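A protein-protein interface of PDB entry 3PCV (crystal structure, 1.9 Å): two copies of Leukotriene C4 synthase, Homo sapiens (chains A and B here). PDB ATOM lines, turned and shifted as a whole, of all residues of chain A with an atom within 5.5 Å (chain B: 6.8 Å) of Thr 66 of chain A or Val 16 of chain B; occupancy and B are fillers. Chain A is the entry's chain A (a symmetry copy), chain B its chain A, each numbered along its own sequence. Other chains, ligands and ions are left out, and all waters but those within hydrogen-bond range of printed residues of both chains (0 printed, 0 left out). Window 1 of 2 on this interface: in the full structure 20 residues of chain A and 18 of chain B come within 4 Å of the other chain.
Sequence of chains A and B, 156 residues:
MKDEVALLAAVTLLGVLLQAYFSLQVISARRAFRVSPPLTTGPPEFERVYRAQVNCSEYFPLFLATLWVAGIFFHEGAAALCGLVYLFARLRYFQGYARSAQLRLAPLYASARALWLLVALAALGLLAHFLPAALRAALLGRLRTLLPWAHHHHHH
The backbone carbonyl oxygen of Leu 62 of chain A sits at hydrogen-bond distance from the side-chain hydroxyl of Thr 66 of chain A (3.1 Å).
OG1 of Thr 66 of chain A lies within hydrogen-bond range of O of Phe 63 of chain A, at 3.3 Å.
Gln 19 of chain B touches Leu 62 of chain A.
Phe 60 of chain B touches Leu 62 of chain A.
Thr 12 of chain B touches Ala 65 of chain A.
Ala 65 of chain A touches Val 16 of chain B.
Val 16 of chain B touches Thr 66 of chain A (CG1 to CG2, 3.5 Å).
Leu 17 of chain B touches Val 119 of chain A (CD2 to CG1, 3.7 Å).
Leu 13 of chain B touches Ala 122 of chain A (CD1 to CB, 3.98 Å).
Printed residues of chain B within 4 Å of Leu 62 of chain A: Gln 19 and Phe 60.
Phe 63 of chain A touches none of the printed residues of chain B.
Val 69 of chain A touches none of the printed residues of chain B.
Of the printed residues of chain A, Val 16 of chain B touches Ala 65 and Thr 66.
Of the printed residues of chain A, Gln 19 of chain B touches Leu 62.
Printed residues of chain B that touch a printed residue of chain A: Thr 12, Leu 13, Val 16, Leu 17, Gln 19 and Phe 60.
Hydrophobic or aromatic side chains of chain B that line the printed part of chain A: Leu 13, Val 16, Leu 17 and Phe 60.
Of the 15 printed residues of chain A, 5 touch a printed residue of chain B.
Printed residues of chain A that touch a printed residue of chain B: Leu 62, Ala 65, Thr 66, Val 119 and Ala 122.
Among the printed residues, 7 pairs touch across the chains.
Among the printed residues, no Asp or Glu carboxylate lies within 4 Å of a Lys or Arg side-chain nitrogen of the other chain.
Position printed for both chains: 64.
Of the 7 pairs that touch across the chains among the printed residues, none has its exchanged pair printed and touching as well.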
ATOM      1  N   PRO A  61       6.002 -27.288  26.976  1.00  0.00           N
ATOM      2  CA  PRO A  61       7.058 -26.627  26.167  1.00  0.00           C
ATOM      3  C   PRO A  61       6.974 -25.106  26.141  1.00  0.00           C
ATOM      4  O   PRO A  61       8.021 -24.444  25.983  1.00  0.00           O
ATOM      5  CB  PRO A  61       6.807 -27.153  24.741  1.00  0.00           C
ATOM      6  CG  PRO A  61       5.982 -28.469  24.956  1.00  0.00           C
ATOM      7  CD  PRO A  61       5.149 -28.188  26.146  1.00  0.00           C
ATOM      8  N   LEU A  62       5.767 -24.544  26.264  1.00  0.00           N
ATOM      9  CA  LEU A  62       5.611 -23.094  26.315  1.00  0.00           C
ATOM     10  C   LEU A  62       6.215 -22.580  27.585  1.00  0.00           C
ATOM     11  O   LEU A  62       6.876 -21.522  27.589  1.00  0.00           O
ATOM     12  CB  LEU A  62       4.132 -22.650  26.251  1.00  0.00           C
ATOM     13  CG  LEU A  62       3.523 -22.499  24.869  1.00  0.00           C
ATOM     14  CD1 LEU A  62       3.637 -23.780  24.127  1.00  0.00           C
ATOM     15  CD2 LEU A  62       2.056 -22.004  24.952  1.00  0.00           C
ATOM     16  N   PHE A  63       5.935 -23.278  28.675  1.00  0.00           N
ATOM     17  CA  PHE A  63       6.536 -22.936  29.929  1.00  0.00           C
ATOM     18  C   PHE A  63       8.072 -23.036  29.869  1.00  0.00           C
ATOM     19  O   PHE A  63       8.767 -22.092  30.293  1.00  0.00           O
ATOM     20  CB  PHE A  63       5.972 -23.803  31.045  1.00  0.00           C
ATOM     21  CG  PHE A  63       6.683 -23.643  32.317  1.00  0.00           C
ATOM     22  CD1 PHE A  63       6.739 -22.405  32.927  1.00  0.00           C
ATOM     23  CD2 PHE A  63       7.335 -24.716  32.904  1.00  0.00           C
ATOM     24  CE1 PHE A  63       7.417 -22.249  34.108  1.00  0.00           C
ATOM     25  CE2 PHE A  63       8.005 -24.556  34.078  1.00  0.00           C
ATOM     26  CZ  PHE A  63       8.042 -23.323  34.686  1.00  0.00           C
ATOM     27  N   LEU A  64       8.597 -24.141  29.349  1.00  0.00           N
ATOM     28  CA  LEU A  64      10.077 -24.253  29.248  1.00  0.00           C
ATOM     29  C   LEU A  64      10.688 -23.143  28.385  1.00  0.00           C
ATOM     30  O   LEU A  64      11.704 -22.517  28.777  1.00  0.00           O
ATOM     31  CB  LEU A  64      10.472 -25.587  28.633  1.00  0.00           C
ATOM     32  CG  LEU A  64      10.197 -26.876  29.432  1.00  0.00           C
ATOM     33  CD1 LEU A  64      10.616 -28.091  28.600  1.00  0.00           C
ATOM     34  CD2 LEU A  64      10.846 -26.897  30.800  1.00  0.00           C
ATOM     35  N   ALA A  65      10.122 -22.922  27.206  1.00  0.00           N
ATOM     36  CA  ALA A  65      10.662 -21.897  26.280  1.00  0.00           C
ATOM     37  C   ALA A  65      10.686 -20.502  26.930  1.00  0.00           C
ATOM     38  O   ALA A  65      11.702 -19.779  26.842  1.00  0.00           O
ATOM     39  CB  ALA A  65       9.840 -21.857  24.968  1.00  0.00           C
ATOM     40  N   THR A  66       9.583 -20.131  27.589  1.00  0.00           N
ATOM     41  CA  THR A  66       9.470 -18.810  28.199  1.00  0.00           C
ATOM     42  C   THR A  66      10.328 -18.670  29.432  1.00  0.00           C
ATOM     43  O   THR A  66      10.910 -17.606  29.647  1.00  0.00           O
ATOM     44  CB  THR A  66       8.012 -18.357  28.540  1.00  0.00           C
ATOM     45  OG1 THR A  66       7.428 -19.213  29.535  1.00  0.00           O
ATOM     46  CG2 THR A  66       7.157 -18.304  27.271  1.00  0.00           C
ATOM     47  N   LEU A  67      10.381 -19.733  30.238  1.00  0.00           N
ATOM     48  CA  LEU A  67      11.214 -19.764  31.433  1.00  0.00           C
ATOM     49  C   LEU A  67      12.684 -19.420  31.044  1.00  0.00           C
ATOM     50  O   LEU A  67      13.339 -18.592  31.696  1.00  0.00           O
ATOM     51  CB  LEU A  67      11.169 -21.147  32.088  1.00  0.00           C
ATOM     52  CG  LEU A  67      12.131 -21.461  33.237  1.00  0.00           C
ATOM     53  CD1 LEU A  67      11.826 -20.535  34.425  1.00  0.00           C
ATOM     54  CD2 LEU A  67      12.100 -22.951  33.668  1.00  0.00           C
ATOM     55  N   TRP A  68      13.194 -20.106  30.027  1.00  0.00           N
ATOM     56  CA  TRP A  68      14.609 -19.957  29.643  1.00  0.00           C
ATOM     57  C   TRP A  68      14.868 -18.599  28.989  1.00  0.00           C
ATOM     58  O   TRP A  68      15.872 -17.939  29.324  1.00  0.00           O
ATOM     59  CB  TRP A  68      15.061 -21.128  28.755  1.00  0.00           C
ATOM     60  CG  TRP A  68      15.304 -22.343  29.614  1.00  0.00           C
ATOM     61  CD1 TRP A  68      14.378 -23.292  30.031  1.00  0.00           C
ATOM     62  CD2 TRP A  68      16.533 -22.674  30.258  1.00  0.00           C
ATOM     63  NE1 TRP A  68      14.990 -24.201  30.867  1.00  0.00           N
ATOM     64  CE2 TRP A  68      16.315 -23.848  31.012  1.00  0.00           C
ATOM     65  CE3 TRP A  68      17.822 -22.089  30.252  1.00  0.00           C
ATOM     66  CZ2 TRP A  68      17.341 -24.468  31.758  1.00  0.00           C
ATOM     67  CZ3 TRP A  68      18.838 -22.706  30.992  1.00  0.00           C
ATOM     68  CH2 TRP A  68      18.590 -23.887  31.726  1.00  0.00           C
ATOM     69  N   VAL A  69      13.988 -18.175  28.079  1.00  0.00           N
ATOM     70  CA  VAL A  69      14.144 -16.840  27.454  1.00  0.00           C
ATOM     71  C   VAL A  69      14.049 -15.700  28.484  1.00  0.00           C
ATOM     72  O   VAL A  69      14.913 -14.780  28.504  1.00  0.00           O
ATOM     73  CB  VAL A  69      13.189 -16.617  26.261  1.00  0.00           C
ATOM     74  CG1 VAL A  69      13.309 -15.192  25.718  1.00  0.00           C
ATOM     75  CG2 VAL A  69      13.468 -17.630  25.132  1.00  0.00           C
ATOM     76  N   ALA A  70      13.037 -15.751  29.357  1.00  0.00           N
ATOM     77  CA  ALA A  70      12.894 -14.733  30.397  1.00  0.00           C
ATOM     78  C   ALA A  70      14.095 -14.771  31.357  1.00  0.00           C
ATOM     79  O   ALA A  70      14.581 -13.707  31.817  1.00  0.00           O
ATOM     80  CB  ALA A  70      11.586 -14.926  31.196  1.00  0.00           C
ATOM     81  N   GLY A  71      14.554 -15.979  31.674  1.00  0.00           N
ATOM     82  CA  GLY A  71      15.612 -16.146  32.663  1.00  0.00           C
ATOM     83  C   GLY A  71      16.957 -15.660  32.126  1.00  0.00           C
ATOM     84  O   GLY A  71      17.816 -15.196  32.888  1.00  0.00           O
ATOM     85  N   LEU A 115       2.224 -17.577  33.394  1.00  0.00           N
ATOM     86  CA  LEU A 115       2.823 -17.767  32.079  1.00  0.00           C
ATOM     87  C   LEU A 115       2.846 -16.460  31.298  1.00  0.00           C
ATOM     88  O   LEU A 115       3.844 -16.152  30.619  1.00  0.00           O
ATOM     89  CB  LEU A 115       2.111 -18.906  31.313  1.00  0.00           C
ATOM     90  CG  LEU A 115       2.696 -19.484  30.028  1.00  0.00           C
ATOM     91  CD1 LEU A 115       4.171 -19.914  30.217  1.00  0.00           C
ATOM     92  CD2 LEU A 115       1.842 -20.711  29.579  1.00  0.00           C
ATOM     93  N   LEU A 118       5.766 -14.486  32.502  1.00  0.00           N
ATOM     94  CA  LEU A 118       7.005 -14.982  31.876  1.00  0.00           C
ATOM     95  C   LEU A 118       7.132 -14.479  30.452  1.00  0.00           C
ATOM     96  O   LEU A 118       8.232 -14.101  30.002  1.00  0.00           O
ATOM     97  CB  LEU A 118       7.089 -16.527  31.902  1.00  0.00           C
ATOM     98  CG  LEU A 118       7.492 -17.154  33.220  1.00  0.00           C
ATOM     99  CD1 LEU A 118       7.271 -18.671  33.184  1.00  0.00           C
ATOM    100  CD2 LEU A 118       8.969 -16.830  33.533  1.00  0.00           C
ATOM    101  N   VAL A 119       6.025 -14.499  29.713  1.00  0.00           N
ATOM    102  CA  VAL A 119       6.032 -14.005  28.342  1.00  0.00           C
ATOM    103  C   VAL A 119       6.412 -12.520  28.338  1.00  0.00           C
ATOM    104  O   VAL A 119       7.224 -12.074  27.522  1.00  0.00           O
ATOM    105  CB  VAL A 119       4.663 -14.227  27.633  1.00  0.00           C
ATOM    106  CG1 VAL A 119       4.590 -13.449  26.342  1.00  0.00           C
ATOM    107  CG2 VAL A 119       4.448 -15.719  27.341  1.00  0.00           C
ATOM    108  N   ALA A 122      10.124 -12.094  29.155  1.00  0.00           N
ATOM    109  CA  ALA A 122      10.903 -12.488  27.984  1.00  0.00           C
ATOM    110  C   ALA A 122      10.855 -11.385  26.897  1.00  0.00           C
ATOM    111  O   ALA A 122      11.877 -11.068  26.258  1.00  0.00           O
ATOM    112  CB  ALA A 122      10.376 -13.816  27.413  1.00  0.00           C
ATOM    113  N   VAL B  11      12.518 -15.649  17.856  1.00  0.00           N
ATOM    114  CA  VAL B  11      11.660 -16.552  17.082  1.00  0.00           C
ATOM    115  C   VAL B  11      10.958 -17.552  18.038  1.00  0.00           C
ATOM    116  O   VAL B  11       9.786 -17.930  17.830  1.00  0.00           O
ATOM    117  CB  VAL B  11      12.448 -17.265  15.979  1.00  0.00           C
ATOM    118  CG1 VAL B  11      11.585 -18.389  15.286  1.00  0.00           C
ATOM    119  CG2 VAL B  11      12.953 -16.237  14.935  1.00  0.00           C
ATOM    120  N   THR B  12      11.670 -17.969  19.078  1.00  0.00           N
ATOM    121  CA  THR B  12      11.095 -18.853  20.116  1.00  0.00           C
ATOM    122  C   THR B  12       9.886 -18.183  20.785  1.00  0.00           C
ATOM    123  O   THR B  12       8.805 -18.780  20.936  1.00  0.00           O
ATOM    124  CB  THR B  12      12.152 -19.224  21.179  1.00  0.00           C
ATOM    125  OG1 THR B  12      13.176 -20.018  20.572  1.00  0.00           O
ATOM    126  CG2 THR B  12      11.518 -20.027  22.331  1.00  0.00           C
ATOM    127  N   LEU B  13      10.049 -16.921  21.165  1.00  0.00           N
ATOM    128  CA  LEU B  13       8.960 -16.203  21.820  1.00  0.00           C
ATOM    129  C   LEU B  13       7.773 -15.992  20.867  1.00  0.00           C
ATOM    130  O   LEU B  13       6.603 -16.092  21.280  1.00  0.00           O
ATOM    131  CB  LEU B  13       9.435 -14.855  22.379  1.00  0.00           C
ATOM    132  CG  LEU B  13       8.377 -14.104  23.222  1.00  0.00           C
ATOM    133  CD1 LEU B  13       7.957 -14.919  24.450  1.00  0.00           C
ATOM    134  CD2 LEU B  13       8.920 -12.730  23.653  1.00  0.00           C
ATOM    135  N   LEU B  14       8.061 -15.689  19.610  1.00  0.00           N
ATOM    136  CA  LEU B  14       7.002 -15.544  18.632  1.00  0.00           C
ATOM    137  C   LEU B  14       6.215 -16.854  18.524  1.00  0.00           C
ATOM    138  O   LEU B  14       4.982 -16.835  18.397  1.00  0.00           O
ATOM    139  CB  LEU B  14       7.598 -15.205  17.267  1.00  0.00           C
ATOM    140  CG  LEU B  14       6.561 -15.002  16.158  1.00  0.00           C
ATOM    141  CD1 LEU B  14       5.590 -13.873  16.523  1.00  0.00           C
ATOM    142  CD2 LEU B  14       7.251 -14.704  14.828  1.00  0.00           C
ATOM    143  N   GLY B  15       6.937 -17.976  18.542  1.00  0.00           N
ATOM    144  CA  GLY B  15       6.302 -19.312  18.502  1.00  0.00           C
ATOM    145  C   GLY B  15       5.390 -19.524  19.711  1.00  0.00           C
ATOM    146  O   GLY B  15       4.290 -20.088  19.584  1.00  0.00           O
ATOM    147  N   VAL B  16       5.840 -19.111  20.892  1.00  0.00           N
ATOM    148  CA  VAL B  16       5.026 -19.215  22.103  1.00  0.00           C
ATOM    149  C   VAL B  16       3.745 -18.383  21.965  1.00  0.00           C
ATOM    150  O   VAL B  16       2.640 -18.828  22.325  1.00  0.00           O
ATOM    151  CB  VAL B  16       5.813 -18.772  23.375  1.00  0.00           C
ATOM    152  CG1 VAL B  16       4.881 -18.682  24.579  1.00  0.00           C
ATOM    153  CG2 VAL B  16       6.951 -19.788  23.693  1.00  0.00           C
ATOM    154  N   LEU B  17       3.895 -17.161  21.471  1.00  0.00           N
ATOM    155  CA  LEU B  17       2.728 -16.290  21.302  1.00  0.00           C
ATOM    156  C   LEU B  17       1.728 -16.892  20.319  1.00  0.00           C
ATOM    157  O   LEU B  17       0.513 -16.793  20.519  1.00  0.00           O
ATOM    158  CB  LEU B  17       3.153 -14.908  20.795  1.00  0.00           C
ATOM    159  CG  LEU B  17       3.913 -14.107  21.861  1.00  0.00           C
ATOM    160  CD1 LEU B  17       4.537 -12.829  21.223  1.00  0.00           C
ATOM    161  CD2 LEU B  17       3.003 -13.746  23.012  1.00  0.00           C
ATOM    162  N   LEU B  18       2.229 -17.496  19.257  1.00  0.00           N
ATOM    163  CA  LEU B  18       1.359 -18.128  18.265  1.00  0.00           C
ATOM    164  C   LEU B  18       0.602 -19.308  18.884  1.00  0.00           C
ATOM    165  O   LEU B  18      -0.613 -19.497  18.635  1.00  0.00           O
ATOM    166  CB  LEU B  18       2.186 -18.618  17.091  1.00  0.00           C
ATOM    167  CG  LEU B  18       1.422 -19.248  15.924  1.00  0.00           C
ATOM    168  CD1 LEU B  18       0.427 -18.244  15.290  1.00  0.00           C
ATOM    169  CD2 LEU B  18       2.381 -19.835  14.867  1.00  0.00           C
ATOM    170  N   GLN B  19       1.314 -20.124  19.664  1.00  0.00           N
ATOM    171  CA  GLN B  19       0.660 -21.249  20.368  1.00  0.00           C
ATOM    172  C   GLN B  19      -0.384 -20.717  21.343  1.00  0.00           C
ATOM    173  O   GLN B  19      -1.437 -21.341  21.518  1.00  0.00           O
ATOM    174  CB  GLN B  19       1.669 -22.155  21.121  1.00  0.00           C
ATOM    175  CG  GLN B  19       2.573 -22.969  20.177  1.00  0.00           C
ATOM    176  CD  GLN B  19       1.770 -24.032  19.401  1.00  0.00           C
ATOM    177  OE1 GLN B  19       0.841 -24.643  19.935  1.00  0.00           O
ATOM    178  NE2 GLN B  19       2.087 -24.197  18.155  1.00  0.00           N
ATOM    179  N   ALA B  20      -0.103 -19.593  22.003  1.00  0.00           N
ATOM    180  CA  ALA B  20      -1.113 -18.993  22.896  1.00  0.00           C
ATOM    181  C   ALA B  20      -2.371 -18.570  22.117  1.00  0.00           C
ATOM    182  O   ALA B  20      -3.511 -18.746  22.579  1.00  0.00           O
ATOM    183  CB  ALA B  20      -0.517 -17.783  23.684  1.00  0.00           C
ATOM    184  N   TYR B  21      -2.155 -18.017  20.936  1.00  0.00           N
ATOM    185  CA  TYR B  21      -3.244 -17.635  20.049  1.00  0.00           C
ATOM    186  C   TYR B  21      -4.093 -18.866  19.674  1.00  0.00           C
ATOM    187  O   TYR B  21      -5.324 -18.827  19.754  1.00  0.00           O
ATOM    188  CB  TYR B  21      -2.683 -16.945  18.798  1.00  0.00           C
ATOM    189  CG  TYR B  21      -3.745 -16.722  17.756  1.00  0.00           C
ATOM    190  CD1 TYR B  21      -4.764 -15.791  17.965  1.00  0.00           C
ATOM    191  CD2 TYR B  21      -3.754 -17.462  16.594  1.00  0.00           C
ATOM    192  CE1 TYR B  21      -5.758 -15.595  17.005  1.00  0.00           C
ATOM    193  CE2 TYR B  21      -4.737 -17.286  15.641  1.00  0.00           C
ATOM    194  CZ  TYR B  21      -5.732 -16.350  15.855  1.00  0.00           C
ATOM    195  OH  TYR B  21      -6.710 -16.180  14.889  1.00  0.00           O
ATOM    196  N   PHE B  60       5.540 -28.413  18.030  1.00  0.00           N
ATOM    197  CA  PHE B  60       6.211 -27.221  18.562  1.00  0.00           C
ATOM    198  C   PHE B  60       7.590 -27.552  19.214  1.00  0.00           C
ATOM    199  O   PHE B  60       8.557 -26.842  18.952  1.00  0.00           O
ATOM    200  CB  PHE B  60       5.275 -26.437  19.493  1.00  0.00           C
ATOM    201  CG  PHE B  60       5.844 -25.110  19.958  1.00  0.00           C
ATOM    202  CD1 PHE B  60       6.036 -24.065  19.065  1.00  0.00           C
ATOM    203  CD2 PHE B  60       6.145 -24.922  21.272  1.00  0.00           C
ATOM    204  CE1 PHE B  60       6.564 -22.866  19.487  1.00  0.00           C
ATOM    205  CE2 PHE B  60       6.669 -23.691  21.720  1.00  0.00           C
ATOM    206  CZ  PHE B  60       6.861 -22.684  20.826  1.00  0.00           C
ATOM    207  N   LEU B  64      11.212 -26.093  18.147  1.00  0.00           N
ATOM    208  CA  LEU B  64      12.182 -25.472  19.088  1.00  0.00           C
ATOM    209  C   LEU B  64      13.544 -26.177  19.071  1.00  0.00           C
ATOM    210  O   LEU B  64      14.606 -25.509  19.016  1.00  0.00           O
ATOM    211  CB  LEU B  64      11.653 -25.522  20.514  1.00  0.00           C
ATOM    212  CG  LEU B  64      10.414 -24.678  20.868  1.00  0.00           C
ATOM    213  CD1 LEU B  64      10.026 -24.930  22.328  1.00  0.00           C
ATOM    214  CD2 LEU B  64      10.584 -23.198  20.594  1.00  0.00           C
ATOM    215  N   LEU B  87       6.731 -20.729  11.278  1.00  0.00           N
ATOM    216  CA  LEU B  87       5.672 -20.218  12.125  1.00  0.00           C
ATOM    217  C   LEU B  87       4.539 -19.560  11.301  1.00  0.00           C
ATOM    218  O   LEU B  87       3.353 -19.673  11.641  1.00  0.00           O
ATOM    219  CB  LEU B  87       6.226 -19.218  13.154  1.00  0.00           C
ATOM    220  CG  LEU B  87       7.128 -19.834  14.255  1.00  0.00           C
ATOM    221  CD1 LEU B  87       7.637 -18.684  15.141  1.00  0.00           C
ATOM    222  CD2 LEU B  87       6.326 -20.866  15.125  1.00  0.00           C
